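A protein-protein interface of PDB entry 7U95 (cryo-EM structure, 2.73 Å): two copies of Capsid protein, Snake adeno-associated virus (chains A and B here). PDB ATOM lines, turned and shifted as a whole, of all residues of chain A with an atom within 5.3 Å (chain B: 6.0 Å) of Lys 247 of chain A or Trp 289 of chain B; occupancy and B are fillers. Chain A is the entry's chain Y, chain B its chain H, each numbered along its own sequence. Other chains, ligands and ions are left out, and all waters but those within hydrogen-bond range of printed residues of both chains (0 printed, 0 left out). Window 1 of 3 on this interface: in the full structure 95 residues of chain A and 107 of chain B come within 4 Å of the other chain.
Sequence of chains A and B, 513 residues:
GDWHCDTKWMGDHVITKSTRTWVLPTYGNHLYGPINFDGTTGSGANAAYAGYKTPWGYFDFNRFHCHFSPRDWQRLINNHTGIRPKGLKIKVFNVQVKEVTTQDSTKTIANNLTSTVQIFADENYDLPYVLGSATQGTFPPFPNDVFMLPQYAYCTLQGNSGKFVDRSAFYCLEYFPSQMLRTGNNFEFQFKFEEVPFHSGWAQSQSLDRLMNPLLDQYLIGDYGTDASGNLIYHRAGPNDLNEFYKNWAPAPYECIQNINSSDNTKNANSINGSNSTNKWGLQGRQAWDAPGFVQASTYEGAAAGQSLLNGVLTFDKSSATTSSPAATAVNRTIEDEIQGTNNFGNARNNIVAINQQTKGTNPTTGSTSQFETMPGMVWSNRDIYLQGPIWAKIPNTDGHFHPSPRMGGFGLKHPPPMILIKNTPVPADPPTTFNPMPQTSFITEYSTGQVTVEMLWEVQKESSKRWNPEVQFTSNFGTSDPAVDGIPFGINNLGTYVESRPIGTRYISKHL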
ATOM      1  N   LEU A 208       1.360 -10.350 -34.070  1.00  0.00           N
ATOM      2  CA  LEU A 208       1.097  -9.397 -32.998  1.00  0.00           C
ATOM      3  C   LEU A 208       0.896 -10.094 -31.668  1.00  0.00           C
ATOM      4  O   LEU A 208       1.297  -9.575 -30.624  1.00  0.00           O
ATOM      5  CB  LEU A 208      -0.125  -8.546 -33.312  1.00  0.00           C
ATOM      6  CG  LEU A 208      -0.025  -7.474 -34.376  1.00  0.00           C
ATOM      7  CD1 LEU A 208      -1.371  -6.855 -34.519  1.00  0.00           C
ATOM      8  CD2 LEU A 208       0.979  -6.439 -33.951  1.00  0.00           C
ATOM      9  N   ASP A 209       0.253 -11.258 -31.674  1.00  0.00           N
ATOM     10  CA  ASP A 209      -0.031 -11.897 -30.406  1.00  0.00           C
ATOM     11  C   ASP A 209       1.216 -12.457 -29.752  1.00  0.00           C
ATOM     12  O   ASP A 209       1.178 -12.744 -28.556  1.00  0.00           O
ATOM     13  CB  ASP A 209      -1.086 -12.986 -30.569  1.00  0.00           C
ATOM     14  CG  ASP A 209      -0.695 -14.039 -31.563  1.00  0.00           C
ATOM     15  OD1 ASP A 209       0.332 -13.873 -32.238  1.00  0.00           O
ATOM     16  OD2 ASP A 209      -1.424 -15.043 -31.674  1.00  0.00           O
ATOM     17  N   MET A 212       6.425 -10.695 -27.452  1.00  0.00           N
ATOM     18  CA  MET A 212       7.014 -10.748 -26.129  1.00  0.00           C
ATOM     19  C   MET A 212       8.286 -11.586 -26.093  1.00  0.00           C
ATOM     20  O   MET A 212       8.556 -12.400 -26.976  1.00  0.00           O
ATOM     21  CB  MET A 212       5.981 -11.316 -25.177  1.00  0.00           C
ATOM     22  CG  MET A 212       5.541 -12.667 -25.646  1.00  0.00           C
ATOM     23  SD  MET A 212       3.955 -13.114 -25.000  1.00  0.00           S
ATOM     24  CE  MET A 212       2.927 -12.227 -26.139  1.00  0.00           C
ATOM     25  N   GLN A 218       4.907 -11.212 -16.984  1.00  0.00           N
ATOM     26  CA  GLN A 218       4.629  -9.792 -16.858  1.00  0.00           C
ATOM     27  C   GLN A 218       4.646  -9.324 -15.414  1.00  0.00           C
ATOM     28  O   GLN A 218       4.439 -10.090 -14.473  1.00  0.00           O
ATOM     29  CB  GLN A 218       3.277  -9.457 -17.458  1.00  0.00           C
ATOM     30  CG  GLN A 218       3.245  -9.465 -18.940  1.00  0.00           C
ATOM     31  CD  GLN A 218       1.882  -9.165 -19.464  1.00  0.00           C
ATOM     32  OE1 GLN A 218       0.886  -9.484 -18.831  1.00  0.00           O
ATOM     33  NE2 GLN A 218       1.823  -8.509 -20.606  1.00  0.00           N
ATOM     34  N   GLY A 222      -3.427  -9.811 -13.979  1.00  0.00           N
ATOM     35  CA  GLY A 222      -4.686  -9.923 -14.675  1.00  0.00           C
ATOM     36  C   GLY A 222      -5.825 -10.312 -13.752  1.00  0.00           C
ATOM     37  O   GLY A 222      -5.647 -10.560 -12.561  1.00  0.00           O
ATOM     38  N   ASP A 223      -7.020 -10.359 -14.325  1.00  0.00           N
ATOM     39  CA  ASP A 223      -8.232 -10.715 -13.596  1.00  0.00           C
ATOM     40  C   ASP A 223      -8.628 -12.114 -14.030  1.00  0.00           C
ATOM     41  O   ASP A 223      -9.082 -12.312 -15.159  1.00  0.00           O
ATOM     42  CB  ASP A 223      -9.353  -9.719 -13.872  1.00  0.00           C
ATOM     43  CG  ASP A 223      -9.047  -8.347 -13.337  1.00  0.00           C
ATOM     44  OD1 ASP A 223      -8.134  -8.233 -12.500  1.00  0.00           O
ATOM     45  OD2 ASP A 223      -9.707  -7.379 -13.757  1.00  0.00           O
ATOM     46  N   LEU A 242       0.679 -17.470 -23.083  1.00  0.00           N
ATOM     47  CA  LEU A 242       1.098 -16.190 -23.617  1.00  0.00           C
ATOM     48  C   LEU A 242      -0.048 -15.403 -24.211  1.00  0.00           C
ATOM     49  O   LEU A 242       0.137 -14.236 -24.547  1.00  0.00           O
ATOM     50  CB  LEU A 242       2.172 -16.373 -24.688  1.00  0.00           C
ATOM     51  CG  LEU A 242       3.502 -17.001 -24.309  1.00  0.00           C
ATOM     52  CD1 LEU A 242       4.315 -17.146 -25.552  1.00  0.00           C
ATOM     53  CD2 LEU A 242       4.259 -16.194 -23.306  1.00  0.00           C
ATOM     54  N   ASN A 243      -1.212 -16.017 -24.378  1.00  0.00           N
ATOM     55  CA  ASN A 243      -2.400 -15.294 -24.801  1.00  0.00           C
ATOM     56  C   ASN A 243      -2.972 -14.424 -23.696  1.00  0.00           C
ATOM     57  O   ASN A 243      -3.790 -13.548 -23.975  1.00  0.00           O
ATOM     58  CB  ASN A 243      -3.447 -16.286 -25.290  1.00  0.00           C
ATOM     59  CG  ASN A 243      -3.723 -17.362 -24.286  1.00  0.00           C
ATOM     60  OD1 ASN A 243      -3.580 -17.161 -23.090  1.00  0.00           O
ATOM     61  ND2 ASN A 243      -4.139 -18.512 -24.760  1.00  0.00           N
ATOM     62  N   GLU A 244      -2.559 -14.656 -22.459  1.00  0.00           N
ATOM     63  CA  GLU A 244      -3.010 -13.922 -21.294  1.00  0.00           C
ATOM     64  C   GLU A 244      -2.367 -12.553 -21.187  1.00  0.00           C
ATOM     65  O   GLU A 244      -2.892 -11.693 -20.473  1.00  0.00           O
ATOM     66  CB  GLU A 244      -2.638 -14.717 -20.060  1.00  0.00           C
ATOM     67  CG  GLU A 244      -3.089 -16.139 -20.118  1.00  0.00           C
ATOM     68  CD  GLU A 244      -4.552 -16.343 -19.886  1.00  0.00           C
ATOM     69  OE1 GLU A 244      -5.026 -15.794 -18.881  1.00  0.00           O
ATOM     70  OE2 GLU A 244      -5.199 -17.027 -20.676  1.00  0.00           O
ATOM     71  N   PHE A 245      -1.227 -12.360 -21.850  1.00  0.00           N
ATOM     72  CA  PHE A 245      -0.474 -11.114 -21.791  1.00  0.00           C
ATOM     73  C   PHE A 245      -1.339  -9.915 -22.121  1.00  0.00           C
ATOM     74  O   PHE A 245      -2.200  -9.972 -22.997  1.00  0.00           O
ATOM     75  CB  PHE A 245       0.691 -11.188 -22.775  1.00  0.00           C
ATOM     76  CG  PHE A 245       1.920 -11.838 -22.223  1.00  0.00           C
ATOM     77  CD1 PHE A 245       3.023 -11.080 -21.916  1.00  0.00           C
ATOM     78  CD2 PHE A 245       1.944 -13.168 -21.907  1.00  0.00           C
ATOM     79  CE1 PHE A 245       4.147 -11.648 -21.389  1.00  0.00           C
ATOM     80  CE2 PHE A 245       3.072 -13.728 -21.359  1.00  0.00           C
ATOM     81  CZ  PHE A 245       4.172 -12.968 -21.103  1.00  0.00           C
ATOM     82  N   TYR A 246      -1.106  -8.824 -21.407  1.00  0.00           N
ATOM     83  CA  TYR A 246      -1.590  -7.542 -21.873  1.00  0.00           C
ATOM     84  C   TYR A 246      -0.713  -7.061 -23.017  1.00  0.00           C
ATOM     85  O   TYR A 246       0.486  -7.335 -23.066  1.00  0.00           O
ATOM     86  CB  TYR A 246      -1.600  -6.492 -20.765  1.00  0.00           C
ATOM     87  CG  TYR A 246      -2.574  -6.748 -19.647  1.00  0.00           C
ATOM     88  CD1 TYR A 246      -3.539  -7.720 -19.753  1.00  0.00           C
ATOM     89  CD2 TYR A 246      -2.648  -5.892 -18.577  1.00  0.00           C
ATOM     90  CE1 TYR A 246      -4.460  -7.920 -18.764  1.00  0.00           C
ATOM     91  CE2 TYR A 246      -3.580  -6.070 -17.594  1.00  0.00           C
ATOM     92  CZ  TYR A 246      -4.486  -7.087 -17.696  1.00  0.00           C
ATOM     93  OH  TYR A 246      -5.423  -7.279 -16.714  1.00  0.00           O
ATOM     94  N   LYS A 247      -1.322  -6.341 -23.947  1.00  0.00           N
ATOM     95  CA  LYS A 247      -0.642  -5.962 -25.173  1.00  0.00           C
ATOM     96  C   LYS A 247      -0.993  -4.529 -25.521  1.00  0.00           C
ATOM     97  O   LYS A 247      -2.059  -4.036 -25.157  1.00  0.00           O
ATOM     98  CB  LYS A 247      -1.012  -6.925 -26.300  1.00  0.00           C
ATOM     99  CG  LYS A 247      -0.378  -8.283 -26.118  1.00  0.00           C
ATOM    100  CD  LYS A 247      -0.839  -9.281 -27.125  1.00  0.00           C
ATOM    101  CE  LYS A 247      -2.248  -9.684 -26.845  1.00  0.00           C
ATOM    102  NZ  LYS A 247      -2.322 -10.379 -25.551  1.00  0.00           N
ATOM    103  N   ASN A 248      -0.059  -3.849 -26.185  1.00  0.00           N
ATOM    104  CA  ASN A 248      -0.284  -2.469 -26.590  1.00  0.00           C
ATOM    105  C   ASN A 248      -1.103  -2.342 -27.862  1.00  0.00           C
ATOM    106  O   ASN A 248      -1.712  -1.293 -28.078  1.00  0.00           O
ATOM    107  CB  ASN A 248       1.037  -1.738 -26.818  1.00  0.00           C
ATOM    108  CG  ASN A 248       1.807  -1.517 -25.552  1.00  0.00           C
ATOM    109  OD1 ASN A 248       1.433  -0.707 -24.716  1.00  0.00           O
ATOM    110  ND2 ASN A 248       2.936  -2.195 -25.430  1.00  0.00           N
ATOM    111  N   TRP A 249      -1.094  -3.343 -28.736  1.00  0.00           N
ATOM    112  CA  TRP A 249      -1.612  -3.162 -30.080  1.00  0.00           C
ATOM    113  C   TRP A 249      -2.623  -4.255 -30.387  1.00  0.00           C
ATOM    114  O   TRP A 249      -2.664  -5.291 -29.727  1.00  0.00           O
ATOM    115  CB  TRP A 249      -0.479  -3.175 -31.109  1.00  0.00           C
ATOM    116  CG  TRP A 249       0.641  -2.248 -30.757  1.00  0.00           C
ATOM    117  CD1 TRP A 249       1.887  -2.600 -30.352  1.00  0.00           C
ATOM    118  CD2 TRP A 249       0.584  -0.824 -30.672  1.00  0.00           C
ATOM    119  NE1 TRP A 249       2.630  -1.485 -30.077  1.00  0.00           N
ATOM    120  CE2 TRP A 249       1.848  -0.380 -30.260  1.00  0.00           C
ATOM    121  CE3 TRP A 249      -0.407   0.120 -30.928  1.00  0.00           C
ATOM    122  CZ2 TRP A 249       2.144   0.962 -30.100  1.00  0.00           C
ATOM    123  CZ3 TRP A 249      -0.109   1.442 -30.770  1.00  0.00           C
ATOM    124  CH2 TRP A 249       1.154   1.854 -30.361  1.00  0.00           C
ATOM    125  N   GLY B 274     -12.597 -15.919 -15.680  1.00  0.00           N
ATOM    126  CA  GLY B 274     -12.071 -14.744 -16.344  1.00  0.00           C
ATOM    127  C   GLY B 274     -11.535 -15.014 -17.729  1.00  0.00           C
ATOM    128  O   GLY B 274     -11.438 -14.086 -18.535  1.00  0.00           O
ATOM    129  N   SER B 275     -11.182 -16.260 -18.024  1.00  0.00           N
ATOM    130  CA  SER B 275     -10.692 -16.590 -19.350  1.00  0.00           C
ATOM    131  C   SER B 275     -11.816 -16.661 -20.362  1.00  0.00           C
ATOM    132  O   SER B 275     -11.608 -16.342 -21.535  1.00  0.00           O
ATOM    133  CB  SER B 275      -9.947 -17.919 -19.315  1.00  0.00           C
ATOM    134  OG  SER B 275      -8.826 -17.842 -18.460  1.00  0.00           O
ATOM    135  N   THR B 278     -13.479 -12.714 -20.865  1.00  0.00           N
ATOM    136  CA  THR B 278     -12.647 -11.613 -21.322  1.00  0.00           C
ATOM    137  C   THR B 278     -12.830 -11.388 -22.820  1.00  0.00           C
ATOM    138  O   THR B 278     -13.109 -12.319 -23.576  1.00  0.00           O
ATOM    139  CB  THR B 278     -11.179 -11.896 -21.004  1.00  0.00           C
ATOM    140  OG1 THR B 278     -11.037 -12.115 -19.601  1.00  0.00           O
ATOM    141  CG2 THR B 278     -10.307 -10.729 -21.381  1.00  0.00           C
ATOM    142  N   ASN B 279     -12.696 -10.133 -23.242  1.00  0.00           N
ATOM    143  CA  ASN B 279     -12.658  -9.826 -24.661  1.00  0.00           C
ATOM    144  C   ASN B 279     -11.424 -10.433 -25.307  1.00  0.00           C
ATOM    145  O   ASN B 279     -10.328 -10.385 -24.750  1.00  0.00           O
ATOM    146  CB  ASN B 279     -12.646  -8.322 -24.895  1.00  0.00           C
ATOM    147  CG  ASN B 279     -13.926  -7.664 -24.484  1.00  0.00           C
ATOM    148  OD1 ASN B 279     -14.937  -8.322 -24.293  1.00  0.00           O
ATOM    149  ND2 ASN B 279     -13.903  -6.350 -24.386  1.00  0.00           N
ATOM    150  N   LYS B 280     -11.603 -10.975 -26.501  1.00  0.00           N
ATOM    151  CA  LYS B 280     -10.537 -11.589 -27.270  1.00  0.00           C
ATOM    152  C   LYS B 280     -10.383 -10.838 -28.580  1.00  0.00           C
ATOM    153  O   LYS B 280     -11.296 -10.148 -29.031  1.00  0.00           O
ATOM    154  CB  LYS B 280     -10.851 -13.046 -27.593  1.00  0.00           C
ATOM    155  CG  LYS B 280     -11.247 -13.890 -26.423  1.00  0.00           C
ATOM    156  CD  LYS B 280     -10.121 -14.187 -25.505  1.00  0.00           C
ATOM    157  CE  LYS B 280     -10.653 -14.992 -24.354  1.00  0.00           C
ATOM    158  NZ  LYS B 280     -11.252 -16.247 -24.853  1.00  0.00           N
ATOM    159  N   TRP B 281      -9.221 -10.973 -29.194  1.00  0.00           N
ATOM    160  CA  TRP B 281      -9.092 -10.763 -30.624  1.00  0.00           C
ATOM    161  C   TRP B 281      -8.337 -11.931 -31.221  1.00  0.00           C
ATOM    162  O   TRP B 281      -7.287 -12.325 -30.715  1.00  0.00           O
ATOM    163  CB  TRP B 281      -8.413  -9.444 -31.005  1.00  0.00           C
ATOM    164  CG  TRP B 281      -7.088  -9.108 -30.415  1.00  0.00           C
ATOM    165  CD1 TRP B 281      -6.856  -8.263 -29.387  1.00  0.00           C
ATOM    166  CD2 TRP B 281      -5.809  -9.596 -30.828  1.00  0.00           C
ATOM    167  NE1 TRP B 281      -5.518  -8.175 -29.133  1.00  0.00           N
ATOM    168  CE2 TRP B 281      -4.851  -8.991 -30.004  1.00  0.00           C
ATOM    169  CE3 TRP B 281      -5.380 -10.484 -31.813  1.00  0.00           C
ATOM    170  CZ2 TRP B 281      -3.498  -9.247 -30.131  1.00  0.00           C
ATOM    171  CZ3 TRP B 281      -4.042 -10.734 -31.935  1.00  0.00           C
ATOM    172  CH2 TRP B 281      -3.115 -10.120 -31.103  1.00  0.00           C
ATOM    173  N   GLN B 287      -6.726 -17.151 -30.933  1.00  0.00           N
ATOM    174  CA  GLN B 287      -7.235 -15.894 -30.402  1.00  0.00           C
ATOM    175  C   GLN B 287      -6.640 -15.581 -29.039  1.00  0.00           C
ATOM    176  O   GLN B 287      -6.566 -16.454 -28.172  1.00  0.00           O
ATOM    177  CB  GLN B 287      -8.761 -15.924 -30.343  1.00  0.00           C
ATOM    178  CG  GLN B 287      -9.334 -17.091 -29.614  1.00  0.00           C
ATOM    179  CD  GLN B 287     -10.834 -17.083 -29.648  1.00  0.00           C
ATOM    180  OE1 GLN B 287     -11.438 -16.361 -30.428  1.00  0.00           O
ATOM    181  NE2 GLN B 287     -11.447 -17.910 -28.818  1.00  0.00           N
ATOM    182  N   ALA B 288      -6.230 -14.330 -28.859  1.00  0.00           N
ATOM    183  CA  ALA B 288      -5.528 -13.863 -27.675  1.00  0.00           C
ATOM    184  C   ALA B 288      -6.365 -12.826 -26.946  1.00  0.00           C
ATOM    185  O   ALA B 288      -7.210 -12.159 -27.542  1.00  0.00           O
ATOM    186  CB  ALA B 288      -4.176 -13.253 -28.039  1.00  0.00           C
ATOM    187  N   TRP B 289      -6.129 -12.705 -25.644  1.00  0.00           N
ATOM    188  CA  TRP B 289      -6.828 -11.700 -24.861  1.00  0.00           C
ATOM    189  C   TRP B 289      -6.640 -10.320 -25.459  1.00  0.00           C
ATOM    190  O   TRP B 289      -5.527  -9.934 -25.818  1.00  0.00           O
ATOM    191  CB  TRP B 289      -6.333 -11.678 -23.425  1.00  0.00           C
ATOM    192  CG  TRP B 289      -6.807 -12.793 -22.598  1.00  0.00           C
ATOM    193  CD1 TRP B 289      -7.462 -13.897 -23.009  1.00  0.00           C
ATOM    194  CD2 TRP B 289      -6.774 -12.841 -21.177  1.00  0.00           C
ATOM    195  NE1 TRP B 289      -7.785 -14.673 -21.934  1.00  0.00           N
ATOM    196  CE2 TRP B 289      -7.376 -14.041 -20.791  1.00  0.00           C
ATOM    197  CE3 TRP B 289      -6.262 -11.994 -20.193  1.00  0.00           C
ATOM    198  CZ2 TRP B 289      -7.495 -14.416 -19.467  1.00  0.00           C
ATOM    199  CZ3 TRP B 289      -6.377 -12.376 -18.887  1.00  0.00           C
ATOM    200  CH2 TRP B 289      -6.988 -13.568 -18.535  1.00  0.00           C
ATOM    201  N   ASP B 290      -7.728  -9.568 -25.564  1.00  0.00           N
ATOM    202  CA  ASP B 290      -7.628  -8.145 -25.851  1.00  0.00           C
ATOM    203  C   ASP B 290      -7.636  -7.458 -24.504  1.00  0.00           C
ATOM    204  O   ASP B 290      -8.686  -7.291 -23.882  1.00  0.00           O
ATOM    205  CB  ASP B 290      -8.793  -7.678 -26.713  1.00  0.00           C
ATOM    206  CG  ASP B 290      -8.670  -6.234 -27.119  1.00  0.00           C
ATOM    207  OD1 ASP B 290      -7.646  -5.602 -26.785  1.00  0.00           O
ATOM    208  OD2 ASP B 290      -9.593  -5.724 -27.784  1.00  0.00           O
ATOM    209  N   ALA B 291      -6.469  -7.037 -24.053  1.00  0.00           N
ATOM    210  CA  ALA B 291      -6.390  -6.385 -22.775  1.00  0.00           C
ATOM    211  C   ALA B 291      -5.234  -5.429 -22.777  1.00  0.00           C
ATOM    212  O   ALA B 291      -4.202  -5.726 -23.357  1.00  0.00           O
ATOM    213  CB  ALA B 291      -6.254  -7.399 -21.688  1.00  0.00           C
ATOM    214  N   PRO B 292      -5.381  -4.287 -22.106  1.00  0.00           N
ATOM    215  CA  PRO B 292      -6.587  -3.764 -21.473  1.00  0.00           C
ATOM    216  C   PRO B 292      -7.647  -3.343 -22.482  1.00  0.00           C
ATOM    217  O   PRO B 292      -8.796  -3.135 -22.122  1.00  0.00           O
ATOM    218  CB  PRO B 292      -6.071  -2.550 -20.717  1.00  0.00           C
ATOM    219  CG  PRO B 292      -4.644  -2.806 -20.534  1.00  0.00           C
ATOM    220  CD  PRO B 292      -4.219  -3.451 -21.788  1.00  0.00           C
ATOM    221  N   GLY B 293      -7.249  -3.212 -23.735  1.00  0.00           N
ATOM    222  CA  GLY B 293      -8.133  -2.703 -24.753  1.00  0.00           C
ATOM    223  C   GLY B 293      -8.033  -1.200 -24.831  1.00  0.00           C
ATOM    224  O   GLY B 293      -7.235  -0.561 -24.147  1.00  0.00           O
ATOM    225  N   ASN B 311     -10.307  -7.078 -16.685  1.00  0.00           N
ATOM    226  CA  ASN B 311      -9.177  -6.901 -17.592  1.00  0.00           C
ATOM    227  C   ASN B 311      -9.257  -5.583 -18.351  1.00  0.00           C
ATOM    228  O   ASN B 311      -8.813  -5.485 -19.492  1.00  0.00           O
ATOM    229  CB  ASN B 311      -9.056  -8.072 -18.560  1.00  0.00           C
ATOM    230  CG  ASN B 311      -8.687  -9.349 -17.869  1.00  0.00           C
ATOM    231  OD1 ASN B 311      -9.325 -10.377 -18.057  1.00  0.00           O
ATOM    232  ND2 ASN B 311      -7.643  -9.297 -17.066  1.00  0.00           N
ATOM    233  N   ARG B 407      -1.823   0.882 -25.911  1.00  0.00           N
ATOM    234  CA  ARG B 407      -3.008   0.638 -25.107  1.00  0.00           C
ATOM    235  C   ARG B 407      -2.701   0.448 -23.637  1.00  0.00           C
ATOM    236  O   ARG B 407      -3.595   0.638 -22.809  1.00  0.00           O
ATOM    237  CB  ARG B 407      -3.769  -0.573 -25.631  1.00  0.00           C
ATOM    238  CG  ARG B 407      -4.489  -0.306 -26.917  1.00  0.00           C
ATOM    239  CD  ARG B 407      -5.336  -1.479 -27.287  1.00  0.00           C
ATOM    240  NE  ARG B 407      -6.185  -1.184 -28.429  1.00  0.00           N
ATOM    241  CZ  ARG B 407      -7.029  -2.052 -28.961  1.00  0.00           C
ATOM    242  NH1 ARG B 407      -7.133  -3.266 -28.454  1.00  0.00           N
ATOM    243  NH2 ARG B 407      -7.775  -1.702 -29.992  1.00  0.00           N
ATOM    244  N   MET B 408      -1.480   0.058 -23.285  1.00  0.00           N
ATOM    245  CA  MET B 408      -1.144  -0.015 -21.870  1.00  0.00           C
ATOM    246  C   MET B 408      -0.781   1.352 -21.314  1.00  0.00           C
ATOM    247  O   MET B 408      -1.076   1.644 -20.154  1.00  0.00           O
ATOM    248  CB  MET B 408      -0.016  -1.014 -21.640  1.00  0.00           C
ATOM    249  CG  MET B 408      -0.424  -2.438 -21.921  1.00  0.00           C
ATOM    250  SD  MET B 408       0.789  -3.658 -21.418  1.00  0.00           S
ATOM    251  CE  MET B 408       2.042  -3.472 -22.661  1.00  0.00           C
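Along chain B the printed residues that touch a printed residue of chain A span positions 281 to 408.
Of the 14 printed residues of chain A, 8 touch a printed residue of chain B.
Hydrophobic or aromatic side chains of chain A within 4 Å of the printed part of chain B: Tyr 246.
Among the printed residues, 16 pairs touch across the chains.
Among the printed residues, no Asp or Glu carboxylate lies within 4 Å of a Lys or Arg side-chain nitrogen of the other chain.
Gln 218 of chain A touches none of the printed residues of chain B.
Printed residues of chain B within 4 Å of Gly 222 of chain A: Asn 311.
Of chain B, only Trp 281 (3.5 Å), Trp 289 (3.2 Å), Ala 291 (3.0 Å), Arg 407 (3.9 Å) and Met 408 (3.96 Å) come within 4 Å of Lys 247 of chain A.
Of the printed residues of chain A, Trp 289 of chain B touches Asn 243 (3.0 Å), Glu 244 (2.9 Å) and Lys 247 (3.2 Å).
Pro 292 of chain B touches none of the printed residues of chain A.
Printed residues of chain A within 4 Å of Met 408 of chain B: Tyr 246 (3.8 Å), Lys 247 (3.96 Å) and Asn 248 (3.2 Å).
The nearest printed residue of chain B that does not touch Glu 244 of chain A is Ser 275 of chain B (4.3 Å).
The backbone NH (N) of Trp 289 of chain B sits at hydrogen-bond distance from the backbone carbonyl oxygen (O) of Asn 243 of chain A, at 3.0 Å.
O of Trp 289 of chain B lies within hydrogen-bond range of NZ of Lys 247 of chain A, at 3.2 Å.
The backbone carbonyl oxygen of Ala 291 of chain B lies within hydrogen-bond range of the backbone NH of Lys 247 of chain A (3.0 Å).
N of Asn 311 of chain B sits at hydrogen-bond distance from OD2 of Asp 223 of chain A.
The side-chain amide nitrogen (ND2) of Asn 311 of chain B lies within hydrogen-bond range of the side-chain hydroxyl (OH) of Tyr 246 of chain A (3.0 Å).
N of Arg 407 of chain B lies within hydrogen-bond range of O of Asn 248 of chain A.
N of Met 408 of chain B sits at hydrogen-bond distance from OD1 of Asn 248 of chain A, 3.3 Å away.
Among the printed residues, merely in contact across the chains: Asp 209 of chain A with Trp 281 of chain B (3.6 Å), Gly 222 of chain A with Asn 311 of chain B (3.9 Å), Asn 243 of chain A with Ala 288 of chain B (3.99 Å), Glu 244 of chain A with Trp 289 of chain B (2.9 Å), Tyr 246 of chain A with Ala 291 of chain B (3.3 Å), Tyr 246 of chain A with Met 408 of chain B (3.8 Å), Lys 247 of chain A with Trp 281 of chain B (3.5 Å), Lys 247 of chain A with Arg 407 of chain B (3.9 Å) and Lys 247 of chain A with Met 408 of chain B (3.96 Å).
No position is printed for both chains.
Of the 16 pairs that touch across the chains among the printed residues, none has its exchanged pair printed and touching as well.
The side-chain hydroxyl (OG1) of Thr 278 of chain B sits at hydrogen-bond distance from the side-chain amide oxygen (OD1) of Asn 311 of chain B (2.9 Å).
N of Trp 281 of chain B is in hydrogen-bond range of O of Ala 288 of chain B, at 2.9 Å.
The side-chain carboxylate (OD1) of Asp 290 of chain B lies within salt-bridge range of the guanidinium group (NH1) of Arg 407 of chain B, 2.9 Å away.
The backbone carbonyl oxygen of Tyr 246 of chain A lies within hydrogen-bond range of the side-chain amide nitrogen of Gln 218 of chain A, at 3.0 Å.
The side-chain carboxylate of Glu 244 of chain A sits close to the side-chain amide oxygen of Asn 243 of chain A, 2.9 Å away.
NZ of Lys 247 of chain A lies within hydrogen-bond range of O of Phe 245 of chain A (2.6 Å).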
